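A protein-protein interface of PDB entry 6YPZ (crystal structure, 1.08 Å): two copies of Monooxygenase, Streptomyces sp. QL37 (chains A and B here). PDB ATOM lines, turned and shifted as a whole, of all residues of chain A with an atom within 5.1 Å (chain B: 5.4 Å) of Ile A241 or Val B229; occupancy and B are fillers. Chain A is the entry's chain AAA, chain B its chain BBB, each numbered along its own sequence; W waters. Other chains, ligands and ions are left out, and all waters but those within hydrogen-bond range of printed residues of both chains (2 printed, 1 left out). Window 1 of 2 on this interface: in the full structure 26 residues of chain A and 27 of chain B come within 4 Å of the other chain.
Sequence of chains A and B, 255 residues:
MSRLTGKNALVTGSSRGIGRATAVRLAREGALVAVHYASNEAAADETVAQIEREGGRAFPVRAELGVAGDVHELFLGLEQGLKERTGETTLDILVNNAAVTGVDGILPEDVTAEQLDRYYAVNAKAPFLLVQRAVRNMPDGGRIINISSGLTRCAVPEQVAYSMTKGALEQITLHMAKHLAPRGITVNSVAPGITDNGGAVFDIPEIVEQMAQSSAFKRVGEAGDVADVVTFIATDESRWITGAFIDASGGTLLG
Hydrophobic or aromatic side chains of chain B within 4 Å of the printed part of chain A: Val B229 and Phe B232. Among the printed residues, Asp or Glu carboxylates within 4 Å of a Lys or Arg side-chain nitrogen of the other chain: Arg A239 with Asp B225 (3.0 Å) and Arg A239 with Asp B228 (2.9 Å).
The backbone carbonyl oxygen (O) of Ile A241 lies within hydrogen-bond range of the side-chain amide nitrogen (ND2) of Asn A188 (3.0 Å).
Water W1 lies within hydrogen-bond range of O of Glu A237 (2.8 Å), O of Asp B225 (2.9 Å), N of Trp A240 (3.0 Å) and N of Arg A239 (3.3 Å). Water W2 lies within hydrogen-bond range of the side-chain carboxylate (OD1) of Asp B247 (2.8 Å), the backbone carbonyl oxygen (O) of Trp A240 (2.9 Å), the backbone NH (N) of Thr A242 (3.0 Å) and the backbone NH (N) of Gly B250 (3.3 Å).
Among the printed residues, merely in contact across the chains: Phe A232 with Phe B232 (3.5 Å), Glu A237 with Asp B228 (3.6 Å), Trp A240 with Asp B225 (3.6 Å), Trp A240 with Asp B247 (3.99 Å), Trp A240 with Ala B248 (3.1 Å), Ile A241 with Val B229 (3.9 Å) and Ile A241 with Asp B247 (3.4 Å).
Phe A232 touches its own counterpart, Phe B232. Of the 10 pairs that touch across the chains among the printed residues, 1 has its exchanged pair printed and touching as well.
The guanidinium group of Arg A239 is in salt-bridge range of the side-chain carboxylate of Asp B225 (3.0 Å). The guanidinium group (NH1) of Arg A239 is in salt-bridge range of the side-chain carboxylate (OD2) of Asp B228, 2.9 Å away. O of Trp A240 is in hydrogen-bond range of N of Gly B250, at 2.9 Å.
Ile A241 touches just these residues of chain B: Val B229 and Asp B247. Val B229 touches just one residue of chain A: Ile A241 (3.9 Å). Printed residues of chain B within 4 Å of Arg A239: Asp B225 and Asp B228. Printed residues of chain A within 4 Å of Ala B248: Trp A240 (3.1 Å). Printed residues of chain A within 4 Å of Gly B250: Trp A240 (2.9 Å). Ser A238 touches none of the printed residues of chain B. The nearest residue of chain A that does not touch Val B229 is Glu A237 (4.1 Å). The nearest printed residue of chain A that does not touch Ala B248 is Ile A241 (4.6 Å).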
ATOM      1  N   THR A 186     -19.479 -11.028 -13.916  1.00  0.00           N
ATOM      2  CA  THR A 186     -18.372 -10.131 -13.597  1.00  0.00           C
ATOM      3  C   THR A 186     -17.454 -10.040 -14.786  1.00  0.00           C
ATOM      4  O   THR A 186     -17.334 -10.960 -15.597  1.00  0.00           O
ATOM      5  CB  THR A 186     -17.650 -10.516 -12.361  1.00  0.00           C
ATOM      6  OG1 THR A 186     -16.901 -11.714 -12.606  1.00  0.00           O
ATOM      7  CG2 THR A 186     -18.572 -10.685 -11.181  1.00  0.00           C
ATOM      8  N   ASN A 188     -13.452  -8.561 -15.513  1.00  0.00           N
ATOM      9  CA  ASN A 188     -12.257  -8.081 -14.854  1.00  0.00           C
ATOM     10  C   ASN A 188     -11.067  -8.193 -15.777  1.00  0.00           C
ATOM     11  O   ASN A 188     -11.073  -9.054 -16.682  1.00  0.00           O
ATOM     12  CB  ASN A 188     -11.970  -8.893 -13.598  1.00  0.00           C
ATOM     13  CG  ASN A 188     -12.988  -8.616 -12.529  1.00  0.00           C
ATOM     14  OD1 ASN A 188     -13.064  -7.488 -12.024  1.00  0.00           O
ATOM     15  ND2 ASN A 188     -13.739  -9.628 -12.145  1.00  0.00           N
ATOM     16  N   PHE A 232      -8.705 -18.151  -9.831  1.00  0.00           N
ATOM     17  CA  PHE A 232      -9.493 -17.619  -8.735  1.00  0.00           C
ATOM     18  C   PHE A 232     -10.634 -16.723  -9.240  1.00  0.00           C
ATOM     19  O   PHE A 232     -11.765 -16.805  -8.794  1.00  0.00           O
ATOM     20  CB  PHE A 232      -8.612 -16.843  -7.759  1.00  0.00           C
ATOM     21  CG  PHE A 232      -9.435 -16.040  -6.776  1.00  0.00           C
ATOM     22  CD1 PHE A 232     -10.179 -16.662  -5.818  1.00  0.00           C
ATOM     23  CD2 PHE A 232      -9.565 -14.656  -6.913  1.00  0.00           C
ATOM     24  CE1 PHE A 232     -11.046 -15.936  -4.990  1.00  0.00           C
ATOM     25  CE2 PHE A 232     -10.424 -13.945  -6.076  1.00  0.00           C
ATOM     26  CZ  PHE A 232     -11.113 -14.611  -5.130  1.00  0.00           C
ATOM     27  N   ILE A 233     -10.298 -15.811 -10.176  1.00  0.00           N
ATOM     28  CA  ILE A 233     -11.355 -14.901 -10.664  1.00  0.00           C
ATOM     29  C   ILE A 233     -12.472 -15.700 -11.273  1.00  0.00           C
ATOM     30  O   ILE A 233     -13.658 -15.328 -11.143  1.00  0.00           O
ATOM     31  CB  ILE A 233     -10.738 -13.857 -11.620  1.00  0.00           C
ATOM     32  CG1 ILE A 233      -9.732 -12.953 -10.899  1.00  0.00           C
ATOM     33  CG2 ILE A 233     -11.887 -13.044 -12.243  1.00  0.00           C
ATOM     34  CD1 ILE A 233     -10.296 -12.063  -9.819  1.00  0.00           C
ATOM     35  N   GLU A 237     -15.952 -17.356  -5.520  1.00  0.00           N
ATOM     36  CA  GLU A 237     -15.463 -16.510  -4.421  1.00  0.00           C
ATOM     37  C   GLU A 237     -14.973 -15.136  -4.888  1.00  0.00           C
ATOM     38  O   GLU A 237     -14.709 -14.306  -4.015  1.00  0.00           O
ATOM     39  CB  GLU A 237     -14.383 -17.238  -3.606  1.00  0.00           C
ATOM     40  CG  GLU A 237     -14.949 -18.312  -2.672  1.00  0.00           C
ATOM     41  CD  GLU A 237     -15.526 -19.508  -3.369  1.00  0.00           C
ATOM     42  OE1 GLU A 237     -15.002 -19.990  -4.335  1.00  0.00           O
ATOM     43  OE2 GLU A 237     -16.640 -20.002  -2.928  1.00  0.00           O
ATOM     44  N   SER A 238     -14.883 -14.914  -6.189  1.00  0.00           N
ATOM     45  CA  SER A 238     -14.542 -13.586  -6.702  1.00  0.00           C
ATOM     46  C   SER A 238     -15.782 -12.739  -6.984  1.00  0.00           C
ATOM     47  O   SER A 238     -15.643 -11.687  -7.609  1.00  0.00           O
ATOM     48  CB  SER A 238     -13.735 -13.713  -7.951  1.00  0.00           C
ATOM     49  OG  SER A 238     -14.623 -14.132  -9.004  1.00  0.00           O
ATOM     50  N   ARG A 239     -16.962 -13.183  -6.568  1.00  0.00           N
ATOM     51  CA  ARG A 239     -18.227 -12.570  -7.018  1.00  0.00           C
ATOM     52  C   ARG A 239     -18.280 -11.081  -6.756  1.00  0.00           C
ATOM     53  O   ARG A 239     -19.037 -10.378  -7.469  1.00  0.00           O
ATOM     54  CB  ARG A 239     -19.435 -13.266  -6.383  1.00  0.00           C
ATOM     55  CG  ARG A 239     -19.642 -12.959  -4.891  1.00  0.00           C
ATOM     56  CD  ARG A 239     -20.630 -13.878  -4.229  1.00  0.00           C
ATOM     57  NE  ARG A 239     -20.046 -15.168  -3.885  1.00  0.00           N
ATOM     58  CZ  ARG A 239     -19.229 -15.372  -2.873  1.00  0.00           C
ATOM     59  NH1 ARG A 239     -18.972 -14.405  -1.980  1.00  0.00           N
ATOM     60  NH2 ARG A 239     -18.699 -16.550  -2.705  1.00  0.00           N
ATOM     61  N   TRP A 240     -17.610 -10.588  -5.739  1.00  0.00           N
ATOM     62  CA  TRP A 240     -17.716  -9.175  -5.366  1.00  0.00           C
ATOM     63  C   TRP A 240     -16.621  -8.349  -5.999  1.00  0.00           C
ATOM     64  O   TRP A 240     -16.538  -7.133  -5.710  1.00  0.00           O
ATOM     65  CB  TRP A 240     -17.751  -9.098  -3.836  1.00  0.00           C
ATOM     66  CG  TRP A 240     -18.549  -7.983  -3.303  1.00  0.00           C
ATOM     67  CD1 TRP A 240     -18.082  -7.122  -2.333  1.00  0.00           C
ATOM     68  CD2 TRP A 240     -19.894  -7.657  -3.568  1.00  0.00           C
ATOM     69  NE1 TRP A 240     -19.062  -6.228  -2.028  1.00  0.00           N
ATOM     70  CE2 TRP A 240     -20.152  -6.485  -2.756  1.00  0.00           C
ATOM     71  CE3 TRP A 240     -20.869  -8.195  -4.345  1.00  0.00           C
ATOM     72  CZ2 TRP A 240     -21.392  -5.857  -2.821  1.00  0.00           C
ATOM     73  CZ3 TRP A 240     -22.097  -7.510  -4.415  1.00  0.00           C
ATOM     74  CH2 TRP A 240     -22.324  -6.371  -3.646  1.00  0.00           C
ATOM     75  N   ILE A 241     -15.871  -8.917  -6.924  1.00  0.00           N
ATOM     76  CA  ILE A 241     -14.856  -8.232  -7.750  1.00  0.00           C
ATOM     77  C   ILE A 241     -15.434  -8.083  -9.148  1.00  0.00           C
ATOM     78  O   ILE A 241     -15.589  -9.072  -9.852  1.00  0.00           O
ATOM     79  CB  ILE A 241     -13.538  -8.994  -7.787  1.00  0.00           C
ATOM     80  CG1 ILE A 241     -13.004  -9.293  -6.387  1.00  0.00           C
ATOM     81  CG2 ILE A 241     -12.553  -8.180  -8.614  1.00  0.00           C
ATOM     82  CD1 ILE A 241     -11.752 -10.147  -6.423  1.00  0.00           C
ATOM     83  N   THR A 242     -15.697  -6.833  -9.591  1.00  0.00           N
ATOM     84  CA  THR A 242     -16.048  -6.616 -11.011  1.00  0.00           C
ATOM     85  C   THR A 242     -15.521  -5.278 -11.432  1.00  0.00           C
ATOM     86  O   THR A 242     -15.400  -4.339 -10.608  1.00  0.00           O
ATOM     87  CB  THR A 242     -17.550  -6.759 -11.242  1.00  0.00           C
ATOM     88  OG1 THR A 242     -17.696  -6.958 -12.661  1.00  0.00           O
ATOM     89  CG2 THR A 242     -18.358  -5.558 -10.818  1.00  0.00           C
ATOM     90  N   GLY A 243     -15.243  -5.140 -12.721  1.00  0.00           N
ATOM     91  CA  GLY A 243     -14.703  -3.918 -13.276  1.00  0.00           C
ATOM     92  C   GLY A 243     -13.310  -3.649 -12.851  1.00  0.00           C
ATOM     93  O   GLY A 243     -12.872  -2.463 -12.993  1.00  0.00           O
ATOM     94  N   ALA A 244     -12.566  -4.591 -12.338  1.00  0.00           N
ATOM     95  CA  ALA A 244     -11.303  -4.344 -11.640  1.00  0.00           C
ATOM     96  C   ALA A 244     -10.118  -4.601 -12.527  1.00  0.00           C
ATOM     97  O   ALA A 244     -10.168  -5.405 -13.472  1.00  0.00           O
ATOM     98  CB  ALA A 244     -11.240  -5.230 -10.408  1.00  0.00           C
ATOM     99  N   ILE A 246      -6.684  -6.290 -11.918  1.00  0.00           N
ATOM    100  CA  ILE A 246      -6.015  -7.217 -10.982  1.00  0.00           C
ATOM    101  C   ILE A 246      -4.570  -7.368 -11.414  1.00  0.00           C
ATOM    102  O   ILE A 246      -4.282  -7.938 -12.488  1.00  0.00           O
ATOM    103  CB  ILE A 246      -6.750  -8.566 -10.938  1.00  0.00           C
ATOM    104  CG1 ILE A 246      -8.217  -8.435 -10.597  1.00  0.00           C
ATOM    105  CG2 ILE A 246      -6.025  -9.496  -9.982  1.00  0.00           C
ATOM    106  CD1 ILE A 246      -8.510  -7.870  -9.256  1.00  0.00           C
ATOM    107  N   VAL B 190      -7.238  -4.632   0.278  1.00  0.00           N
ATOM    108  CA  VAL B 190      -8.544  -5.099  -0.177  1.00  0.00           C
ATOM    109  C   VAL B 190      -9.530  -4.020   0.199  1.00  0.00           C
ATOM    110  O   VAL B 190      -9.593  -3.651   1.392  1.00  0.00           O
ATOM    111  CB  VAL B 190      -8.900  -6.458   0.428  1.00  0.00           C
ATOM    112  CG1 VAL B 190     -10.334  -6.837   0.071  1.00  0.00           C
ATOM    113  CG2 VAL B 190      -7.932  -7.519   0.000  1.00  0.00           C
ATOM    114  N   GLY B 224     -19.071 -11.916   4.083  1.00  0.00           N
ATOM    115  CA  GLY B 224     -18.397 -13.011   3.424  1.00  0.00           C
ATOM    116  C   GLY B 224     -17.954 -12.677   2.018  1.00  0.00           C
ATOM    117  O   GLY B 224     -17.000 -13.274   1.525  1.00  0.00           O
ATOM    118  N   ASP B 225     -18.619 -11.735   1.350  1.00  0.00           N
ATOM    119  CA  ASP B 225     -18.196 -11.302  -0.029  1.00  0.00           C
ATOM    120  C   ASP B 225     -16.775 -10.764   0.054  1.00  0.00           C
ATOM    121  O   ASP B 225     -15.952 -10.986  -0.866  1.00  0.00           O
ATOM    122  CB  ASP B 225     -19.135 -10.246  -0.563  1.00  0.00           C
ATOM    123  CG  ASP B 225     -20.496 -10.763  -0.964  1.00  0.00           C
ATOM    124  OD1 ASP B 225     -20.561 -11.860  -1.586  1.00  0.00           O
ATOM    125  OD2 ASP B 225     -21.489 -10.112  -0.628  1.00  0.00           O
ATOM    126  N   VAL B 226     -16.489  -9.946   1.040  1.00  0.00           N
ATOM    127  CA  VAL B 226     -15.165  -9.353   1.251  1.00  0.00           C
ATOM    128  C   VAL B 226     -14.208 -10.387   1.795  1.00  0.00           C
ATOM    129  O   VAL B 226     -13.066 -10.518   1.316  1.00  0.00           O
ATOM    130  CB  VAL B 226     -15.266  -8.132   2.163  1.00  0.00           C
ATOM    131  CG1 VAL B 226     -13.901  -7.546   2.440  1.00  0.00           C
ATOM    132  CG2 VAL B 226     -16.190  -7.066   1.624  1.00  0.00           C
ATOM    133  N   ALA B 227     -14.644 -11.150   2.819  1.00  0.00           N
ATOM    134  CA  ALA B 227     -13.798 -12.127   3.465  1.00  0.00           C
ATOM    135  C   ALA B 227     -13.317 -13.184   2.500  1.00  0.00           C
ATOM    136  O   ALA B 227     -12.234 -13.712   2.626  1.00  0.00           O
ATOM    137  CB  ALA B 227     -14.512 -12.712   4.652  1.00  0.00           C
ATOM    138  N   ASP B 228     -14.141 -13.558   1.524  1.00  0.00           N
ATOM    139  CA  ASP B 228     -13.710 -14.542   0.532  1.00  0.00           C
ATOM    140  C   ASP B 228     -12.523 -14.035  -0.273  1.00  0.00           C
ATOM    141  O   ASP B 228     -11.617 -14.821  -0.646  1.00  0.00           O
ATOM    142  CB  ASP B 228     -14.855 -14.918  -0.431  1.00  0.00           C
ATOM    143  CG  ASP B 228     -15.897 -15.847   0.199  1.00  0.00           C
ATOM    144  OD1 ASP B 228     -15.592 -16.554   1.176  1.00  0.00           O
ATOM    145  OD2 ASP B 228     -17.040 -15.865  -0.369  1.00  0.00           O
ATOM    146  N   VAL B 229     -12.503 -12.739  -0.600  1.00  0.00           N
ATOM    147  CA  VAL B 229     -11.356 -12.156  -1.329  1.00  0.00           C
ATOM    148  C   VAL B 229     -10.113 -12.145  -0.440  1.00  0.00           C
ATOM    149  O   VAL B 229      -9.025 -12.528  -0.860  1.00  0.00           O
ATOM    150  CB  VAL B 229     -11.723 -10.757  -1.841  1.00  0.00           C
ATOM    151  CG1 VAL B 229     -10.531 -10.127  -2.536  1.00  0.00           C
ATOM    152  CG2 VAL B 229     -12.933 -10.823  -2.782  1.00  0.00           C
ATOM    153  N   VAL B 230     -10.285 -11.697   0.805  1.00  0.00           N
ATOM    154  CA  VAL B 230      -9.162 -11.664   1.777  1.00  0.00           C
ATOM    155  C   VAL B 230      -8.559 -13.062   1.891  1.00  0.00           C
ATOM    156  O   VAL B 230      -7.337 -13.233   1.895  1.00  0.00           O
ATOM    157  CB  VAL B 230      -9.624 -11.110   3.136  1.00  0.00           C
ATOM    158  CG1 VAL B 230      -8.501 -11.195   4.149  1.00  0.00           C
ATOM    159  CG2 VAL B 230     -10.117  -9.713   2.989  1.00  0.00           C
ATOM    160  N   THR B 231      -9.424 -14.088   1.996  1.00  0.00           N
ATOM    161  CA  THR B 231      -8.976 -15.463   2.170  1.00  0.00           C
ATOM    162  C   THR B 231      -8.135 -15.900   0.968  1.00  0.00           C
ATOM    163  O   THR B 231      -7.070 -16.501   1.152  1.00  0.00           O
ATOM    164  CB  THR B 231     -10.173 -16.385   2.407  1.00  0.00           C
ATOM    165  OG1 THR B 231     -10.821 -15.988   3.612  1.00  0.00           O
ATOM    166  CG2 THR B 231      -9.770 -17.839   2.536  1.00  0.00           C
ATOM    167  N   PHE B 232      -8.593 -15.620  -0.257  1.00  0.00           N
ATOM    168  CA  PHE B 232      -7.772 -15.947  -1.415  1.00  0.00           C
ATOM    169  C   PHE B 232      -6.414 -15.267  -1.314  1.00  0.00           C
ATOM    170  O   PHE B 232      -5.365 -15.874  -1.578  1.00  0.00           O
ATOM    171  CB  PHE B 232      -8.479 -15.523  -2.695  1.00  0.00           C
ATOM    172  CG  PHE B 232      -7.517 -15.554  -3.864  1.00  0.00           C
ATOM    173  CD1 PHE B 232      -7.038 -16.761  -4.357  1.00  0.00           C
ATOM    174  CD2 PHE B 232      -7.035 -14.388  -4.441  1.00  0.00           C
ATOM    175  CE1 PHE B 232      -6.089 -16.794  -5.392  1.00  0.00           C
ATOM    176  CE2 PHE B 232      -6.076 -14.451  -5.438  1.00  0.00           C
ATOM    177  CZ  PHE B 232      -5.642 -15.623  -5.899  1.00  0.00           C
ATOM    178  N   ILE B 233      -6.387 -13.983  -0.991  1.00  0.00           N
ATOM    179  CA  ILE B 233      -5.070 -13.283  -0.918  1.00  0.00           C
ATOM    180  C   ILE B 233      -4.157 -13.982   0.095  1.00  0.00           C
ATOM    181  O   ILE B 233      -2.952 -14.067  -0.122  1.00  0.00           O
ATOM    182  CB  ILE B 233      -5.273 -11.780  -0.651  1.00  0.00           C
ATOM    183  CG1 ILE B 233      -6.020 -11.140  -1.797  1.00  0.00           C
ATOM    184  CG2 ILE B 233      -3.935 -11.086  -0.431  1.00  0.00           C
ATOM    185  CD1 ILE B 233      -5.357 -11.044  -3.143  1.00  0.00           C
ATOM    186  N   ALA B 234      -4.718 -14.498   1.183  1.00  0.00           N
ATOM    187  CA  ALA B 234      -3.903 -15.184   2.199  1.00  0.00           C
ATOM    188  C   ALA B 234      -3.281 -16.496   1.718  1.00  0.00           C
ATOM    189  O   ALA B 234      -2.402 -17.009   2.402  1.00  0.00           O
ATOM    190  CB  ALA B 234      -4.772 -15.451   3.425  1.00  0.00           C
ATOM    191  N   ILE B 246      -7.012  -4.233  -4.465  1.00  0.00           N
ATOM    192  CA  ILE B 246      -7.981  -5.270  -4.888  1.00  0.00           C
ATOM    193  C   ILE B 246      -9.366  -4.747  -4.558  1.00  0.00           C
ATOM    194  O   ILE B 246      -9.726  -4.589  -3.375  1.00  0.00           O
ATOM    195  CB  ILE B 246      -7.674  -6.598  -4.220  1.00  0.00           C
ATOM    196  CG1 ILE B 246      -6.266  -7.072  -4.496  1.00  0.00           C
ATOM    197  CG2 ILE B 246      -8.729  -7.619  -4.662  1.00  0.00           C
ATOM    198  CD1 ILE B 246      -5.936  -7.388  -5.889  1.00  0.00           C
ATOM    199  N   ASP B 247     -10.155  -4.484  -5.602  1.00  0.00           N
ATOM    200  CA  ASP B 247     -11.501  -3.926  -5.444  1.00  0.00           C
ATOM    201  C   ASP B 247     -12.444  -5.039  -5.042  1.00  0.00           C
ATOM    202  O   ASP B 247     -12.732  -5.937  -5.864  1.00  0.00           O
ATOM    203  CB  ASP B 247     -11.896  -3.274  -6.748  1.00  0.00           C
ATOM    204  CG  ASP B 247     -13.216  -2.621  -6.713  1.00  0.00           C
ATOM    205  OD1 ASP B 247     -14.147  -3.093  -6.032  1.00  0.00           O
ATOM    206  OD2 ASP B 247     -13.310  -1.603  -7.449  1.00  0.00           O
ATOM    207  N   ALA B 248     -12.918  -5.015  -3.825  1.00  0.00           N
ATOM    208  CA  ALA B 248     -13.920  -5.971  -3.324  1.00  0.00           C
ATOM    209  C   ALA B 248     -15.147  -5.193  -2.905  1.00  0.00           C
ATOM    210  O   ALA B 248     -15.653  -5.334  -1.767  1.00  0.00           O
ATOM    211  CB  ALA B 248     -13.381  -6.794  -2.183  1.00  0.00           C
ATOM    212  N   GLY B 250     -18.102  -4.851  -4.976  1.00  0.00           N
ATOM    213  CA  GLY B 250     -19.311  -5.078  -5.763  1.00  0.00           C
ATOM    214  C   GLY B 250     -19.511  -4.033  -6.843  1.00  0.00           C
ATOM    215  O   GLY B 250     -20.692  -3.627  -7.081  1.00  0.00           O
HETATM  216  O   HOH W   1     -16.270 -12.028  -3.535  1.00  0.00           O
HETATM  217  O   HOH W   2     -15.860  -4.881  -7.357  1.00  0.00           O
